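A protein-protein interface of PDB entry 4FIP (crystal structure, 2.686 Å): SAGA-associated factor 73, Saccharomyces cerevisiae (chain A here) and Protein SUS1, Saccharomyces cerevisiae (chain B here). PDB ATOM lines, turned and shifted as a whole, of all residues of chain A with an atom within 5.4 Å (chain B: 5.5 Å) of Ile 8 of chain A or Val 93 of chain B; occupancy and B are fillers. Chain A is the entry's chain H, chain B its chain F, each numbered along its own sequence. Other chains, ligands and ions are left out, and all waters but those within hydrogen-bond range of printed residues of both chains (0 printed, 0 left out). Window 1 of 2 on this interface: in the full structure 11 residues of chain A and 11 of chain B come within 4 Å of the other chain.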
ATOM      1  N   ALA A   6     -25.461 -12.755 -16.705  1.00  0.00           N
ATOM      2  CA  ALA A   6     -24.356 -12.049 -17.429  1.00  0.00           C
ATOM      3  C   ALA A   6     -23.729 -10.980 -16.521  1.00  0.00           C
ATOM      4  O   ALA A   6     -24.359  -9.951 -16.270  1.00  0.00           O
ATOM      5  CB  ALA A   6     -24.886 -11.424 -18.721  1.00  0.00           C
ATOM      6  N   GLU A   7     -22.495 -11.220 -16.052  1.00  0.00           N
ATOM      7  CA  GLU A   7     -21.811 -10.366 -15.037  1.00  0.00           C
ATOM      8  C   GLU A   7     -21.007  -9.174 -15.608  1.00  0.00           C
ATOM      9  O   GLU A   7     -20.138  -9.359 -16.466  1.00  0.00           O
ATOM     10  CB  GLU A   7     -20.851 -11.212 -14.194  1.00  0.00           C
ATOM     11  CG  GLU A   7     -21.468 -12.440 -13.529  1.00  0.00           C
ATOM     12  CD  GLU A   7     -20.478 -13.591 -13.395  1.00  0.00           C
ATOM     13  OE1 GLU A   7     -20.052 -14.145 -14.432  1.00  0.00           O
ATOM     14  OE2 GLU A   7     -20.120 -13.950 -12.254  1.00  0.00           O
ATOM     15  N   ILE A   8     -21.262  -7.965 -15.085  1.00  0.00           N
ATOM     16  CA  ILE A   8     -20.694  -6.710 -15.649  1.00  0.00           C
ATOM     17  C   ILE A   8     -19.190  -6.609 -15.489  1.00  0.00           C
ATOM     18  O   ILE A   8     -18.693  -6.504 -14.370  1.00  0.00           O
ATOM     19  CB  ILE A   8     -21.304  -5.429 -15.013  1.00  0.00           C
ATOM     20  CG1 ILE A   8     -22.776  -5.284 -15.405  1.00  0.00           C
ATOM     21  CG2 ILE A   8     -20.536  -4.183 -15.442  1.00  0.00           C
ATOM     22  CD1 ILE A   8     -23.552  -4.321 -14.533  1.00  0.00           C
ATOM     23  N   LYS A   9     -18.474  -6.599 -16.610  1.00  0.00           N
ATOM     24  CA  LYS A   9     -17.017  -6.540 -16.558  1.00  0.00           C
ATOM     25  C   LYS A   9     -16.456  -5.107 -16.678  1.00  0.00           C
ATOM     26  O   LYS A   9     -15.245  -4.915 -16.622  1.00  0.00           O
ATOM     27  CB  LYS A   9     -16.389  -7.513 -17.583  1.00  0.00           C
ATOM     28  CG  LYS A   9     -16.378  -8.978 -17.119  1.00  0.00           C
ATOM     29  CD  LYS A   9     -15.389  -9.846 -17.895  1.00  0.00           C
ATOM     30  CE  LYS A   9     -15.859 -10.067 -19.321  1.00  0.00           C
ATOM     31  NZ  LYS A   9     -14.912 -10.850 -20.144  1.00  0.00           N
ATOM     32  N   GLY A  10     -17.319  -4.109 -16.819  1.00  0.00           N
ATOM     33  CA  GLY A  10     -16.872  -2.713 -16.825  1.00  0.00           C
ATOM     34  C   GLY A  10     -17.393  -1.946 -18.022  1.00  0.00           C
ATOM     35  O   GLY A  10     -18.038  -2.528 -18.900  1.00  0.00           O
ATOM     36  N   ILE A  11     -17.115  -0.639 -18.049  1.00  0.00           N
ATOM     37  CA  ILE A  11     -17.508   0.245 -19.166  1.00  0.00           C
ATOM     38  C   ILE A  11     -16.634   0.037 -20.396  1.00  0.00           C
ATOM     39  O   ILE A  11     -15.412  -0.076 -20.271  1.00  0.00           O
ATOM     40  CB  ILE A  11     -17.405   1.740 -18.782  1.00  0.00           C
ATOM     41  CG1 ILE A  11     -18.725   2.240 -18.190  1.00  0.00           C
ATOM     42  CG2 ILE A  11     -17.012   2.592 -19.980  1.00  0.00           C
ATOM     43  CD1 ILE A  11     -18.520   3.353 -17.189  1.00  0.00           C
ATOM     44  N   LYS A  12     -17.270  -0.004 -21.571  1.00  0.00           N
ATOM     45  CA  LYS A  12     -16.558  -0.023 -22.850  1.00  0.00           C
ATOM     46  C   LYS A  12     -15.660   1.214 -22.938  1.00  0.00           C
ATOM     47  O   LYS A  12     -16.178   2.332 -23.010  1.00  0.00           O
ATOM     48  CB  LYS A  12     -17.538   0.006 -24.026  1.00  0.00           C
ATOM     49  CG  LYS A  12     -18.348  -1.257 -24.252  1.00  0.00           C
ATOM     50  CD  LYS A  12     -19.277  -1.060 -25.448  1.00  0.00           C
ATOM     51  CE  LYS A  12     -20.388  -2.099 -25.522  1.00  0.00           C
ATOM     52  NZ  LYS A  12     -19.886  -3.501 -25.542  1.00  0.00           N
ATOM     53  N   LEU B   8     -18.957   1.698 -10.051  1.00  0.00           N
ATOM     54  CA  LEU B   8     -19.039   2.500 -11.273  1.00  0.00           C
ATOM     55  C   LEU B   8     -20.477   2.825 -11.635  1.00  0.00           C
ATOM     56  O   LEU B   8     -20.703   3.715 -12.446  1.00  0.00           O
ATOM     57  CB  LEU B   8     -18.360   1.771 -12.443  1.00  0.00           C
ATOM     58  CG  LEU B   8     -19.059   0.601 -13.173  1.00  0.00           C
ATOM     59  CD1 LEU B   8     -18.080   0.008 -14.174  1.00  0.00           C
ATOM     60  CD2 LEU B   8     -19.603  -0.503 -12.270  1.00  0.00           C
ATOM     61  N   ILE B  12     -22.236   4.786 -14.941  1.00  0.00           N
ATOM     62  CA  ILE B  12     -23.234   4.356 -15.925  1.00  0.00           C
ATOM     63  C   ILE B  12     -24.327   5.420 -15.993  1.00  0.00           C
ATOM     64  O   ILE B  12     -24.645   5.953 -17.066  1.00  0.00           O
ATOM     65  CB  ILE B  12     -23.888   3.023 -15.514  1.00  0.00           C
ATOM     66  CG1 ILE B  12     -22.943   1.863 -15.807  1.00  0.00           C
ATOM     67  CG2 ILE B  12     -25.227   2.824 -16.211  1.00  0.00           C
ATOM     68  CD1 ILE B  12     -23.362   0.572 -15.136  1.00  0.00           C
ATOM     69  N   PHE B  88     -30.096  -0.242 -23.162  1.00  0.00           N
ATOM     70  CA  PHE B  88     -29.171   0.899 -23.105  1.00  0.00           C
ATOM     71  C   PHE B  88     -27.800   0.566 -22.475  1.00  0.00           C
ATOM     72  O   PHE B  88     -26.832   1.302 -22.690  1.00  0.00           O
ATOM     73  CB  PHE B  88     -29.801   2.081 -22.361  1.00  0.00           C
ATOM     74  CG  PHE B  88     -30.869   2.805 -23.139  1.00  0.00           C
ATOM     75  CD1 PHE B  88     -30.655   3.205 -24.459  1.00  0.00           C
ATOM     76  CD2 PHE B  88     -32.075   3.135 -22.537  1.00  0.00           C
ATOM     77  CE1 PHE B  88     -31.634   3.898 -25.162  1.00  0.00           C
ATOM     78  CE2 PHE B  88     -33.056   3.827 -23.239  1.00  0.00           C
ATOM     79  CZ  PHE B  88     -32.835   4.210 -24.549  1.00  0.00           C
ATOM     80  N   LEU B  89     -27.726  -0.523 -21.702  1.00  0.00           N
ATOM     81  CA  LEU B  89     -26.457  -0.998 -21.131  1.00  0.00           C
ATOM     82  C   LEU B  89     -25.671  -1.895 -22.091  1.00  0.00           C
ATOM     83  O   LEU B  89     -24.464  -1.723 -22.228  1.00  0.00           O
ATOM     84  CB  LEU B  89     -26.702  -1.747 -19.832  1.00  0.00           C
ATOM     85  CG  LEU B  89     -27.413  -0.956 -18.741  1.00  0.00           C
ATOM     86  CD1 LEU B  89     -27.515  -1.831 -17.506  1.00  0.00           C
ATOM     87  CD2 LEU B  89     -26.713   0.354 -18.424  1.00  0.00           C
ATOM     88  N   GLU B  90     -26.340  -2.846 -22.750  1.00  0.00           N
ATOM     89  CA  GLU B  90     -25.716  -3.595 -23.855  1.00  0.00           C
ATOM     90  C   GLU B  90     -24.965  -2.626 -24.780  1.00  0.00           C
ATOM     91  O   GLU B  90     -23.948  -2.969 -25.358  1.00  0.00           O
ATOM     92  CB  GLU B  90     -26.758  -4.406 -24.656  1.00  0.00           C
ATOM     93  CG  GLU B  90     -26.930  -5.869 -24.237  1.00  0.00           C
ATOM     94  CD  GLU B  90     -26.059  -6.873 -25.024  1.00  0.00           C
ATOM     95  OE1 GLU B  90     -26.042  -8.075 -24.657  1.00  0.00           O
ATOM     96  OE2 GLU B  90     -25.391  -6.493 -26.014  1.00  0.00           O
ATOM     97  N   GLU B  91     -25.472  -1.406 -24.896  1.00  0.00           N
ATOM     98  CA  GLU B  91     -24.856  -0.371 -25.719  1.00  0.00           C
ATOM     99  C   GLU B  91     -23.461   0.054 -25.215  1.00  0.00           C
ATOM    100  O   GLU B  91     -22.493   0.068 -25.996  1.00  0.00           O
ATOM    101  CB  GLU B  91     -25.790   0.847 -25.776  1.00  0.00           C
ATOM    102  CG  GLU B  91     -26.000   1.434 -27.162  1.00  0.00           C
ATOM    103  CD  GLU B  91     -27.232   2.324 -27.237  1.00  0.00           C
ATOM    104  OE1 GLU B  91     -27.539   3.034 -26.249  1.00  0.00           O
ATOM    105  OE2 GLU B  91     -27.904   2.313 -28.288  1.00  0.00           O
ATOM    106  N   ILE B  92     -23.370   0.373 -23.915  1.00  0.00           N
ATOM    107  CA  ILE B  92     -22.166   1.009 -23.311  1.00  0.00           C
ATOM    108  C   ILE B  92     -21.329   0.148 -22.321  1.00  0.00           C
ATOM    109  O   ILE B  92     -20.157   0.438 -22.101  1.00  0.00           O
ATOM    110  CB  ILE B  92     -22.536   2.363 -22.646  1.00  0.00           C
ATOM    111  CG1 ILE B  92     -23.274   2.152 -21.313  1.00  0.00           C
ATOM    112  CG2 ILE B  92     -23.364   3.205 -23.613  1.00  0.00           C
ATOM    113  CD1 ILE B  92     -24.068   3.360 -20.852  1.00  0.00           C
ATOM    114  N   VAL B  93     -21.928  -0.882 -21.722  1.00  0.00           N
ATOM    115  CA  VAL B  93     -21.194  -1.853 -20.895  1.00  0.00           C
ATOM    116  C   VAL B  93     -20.819  -3.039 -21.761  1.00  0.00           C
ATOM    117  O   VAL B  93     -21.449  -3.259 -22.792  1.00  0.00           O
ATOM    118  CB  VAL B  93     -22.044  -2.385 -19.724  1.00  0.00           C
ATOM    119  CG1 VAL B  93     -23.073  -3.392 -20.219  1.00  0.00           C
ATOM    120  CG2 VAL B  93     -21.159  -3.030 -18.664  1.00  0.00           C
ATOM    121  N   ASP B  94     -19.823  -3.818 -21.334  1.00  0.00           N
ATOM    122  CA  ASP B  94     -19.389  -4.992 -22.110  1.00  0.00           C
ATOM    123  C   ASP B  94     -19.252  -6.299 -21.323  1.00  0.00           C
ATOM    124  O   ASP B  94     -19.031  -6.317 -20.102  1.00  0.00           O
ATOM    125  CB  ASP B  94     -18.088  -4.702 -22.864  1.00  0.00           C
ATOM    126  CG  ASP B  94     -17.011  -4.166 -21.971  1.00  0.00           C
ATOM    127  OD1 ASP B  94     -17.162  -4.264 -20.732  1.00  0.00           O
ATOM    128  OD2 ASP B  94     -16.025  -3.637 -22.524  1.00  0.00           O
ATOM    129  N   THR B  95     -19.325  -7.379 -22.102  1.00  0.00           N
ATOM    130  CA  THR B  95     -19.609  -8.729 -21.629  1.00  0.00           C
ATOM    131  C   THR B  95     -18.560  -9.230 -20.641  1.00  0.00           C
ATOM    132  O   THR B  95     -18.681  -9.027 -19.432  1.00  0.00           O
ATOM    133  CB  THR B  95     -19.700  -9.718 -22.820  1.00  0.00           C
ATOM    134  OG1 THR B  95     -18.384 -10.050 -23.278  1.00  0.00           O
ATOM    135  CG2 THR B  95     -20.513  -9.131 -23.990  1.00  0.00           C
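Of the printed residues of chain B, Lys 12 of chain A touches Glu 90, Glu 91, Ile 92, Val 93 and Asp 94.
Printed residues of chain A within 4 Å of Leu 8 of chain B: Gly 10.
Ile 12 of chain B touches none of the printed residues of chain A.
Leu 89 of chain B touches none of the printed residues of chain A.
Printed residues of chain A within 4 Å of Ile 92 of chain B: Ile 11 and Lys 12.
The nearest printed residue of chain B that does not touch Ile 8 of chain A is Asp 94 of chain B (4.6 Å).
The backbone NH (N) of Lys 12 of chain A lies within hydrogen-bond range of the backbone carbonyl oxygen (O) of Ile 92 of chain B, 3.0 Å away.
The side-chain amino group of Lys 12 of chain A sits close to the backbone carbonyl oxygen of Val 93 of chain B (3.2 Å).
The backbone NH of Asp 94 of chain B sits at hydrogen-bond distance from the backbone carbonyl oxygen of Gly 10 of chain A (3.3 Å).
The backbone carbonyl oxygen (O) of Thr 95 of chain B sits close to the backbone carbonyl oxygen (O) of Glu 7 of chain A (3.3 Å).
Printed residues of chain A that touch a printed residue of chain B: Glu 7, Ile 8, Lys 9, Gly 10, Ile 11 and Lys 12.
Hydrophobic or aromatic side chains of chain A that line the printed part of chain B: Ile 8.
Of the 10 printed residues of chain B, 7 touch a printed residue of chain A.
Among the printed residues, 13 pairs touch across the chains.
Among the printed residues, pairs that only touch across the chains: Ile 8 of chain A with Val 93 of chain B (3.5 Å), Lys 9 of chain A with Asp 94 of chain B (3.5 Å), Lys 9 of chain A with Thr 95 of chain B (3.0 Å), Gly 10 of chain A with Leu 8 of chain B (3.99 Å), Gly 10 of chain A with Val 93 of chain B (3.2 Å), Ile 11 of chain A with Ile 92 of chain B (3.9 Å), Lys 12 of chain A with Glu 90 of chain B (3.7 Å), Lys 12 of chain A with Glu 91 of chain B (3.1 Å) and Lys 12 of chain A with Asp 94 of chain B (3.4 Å).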
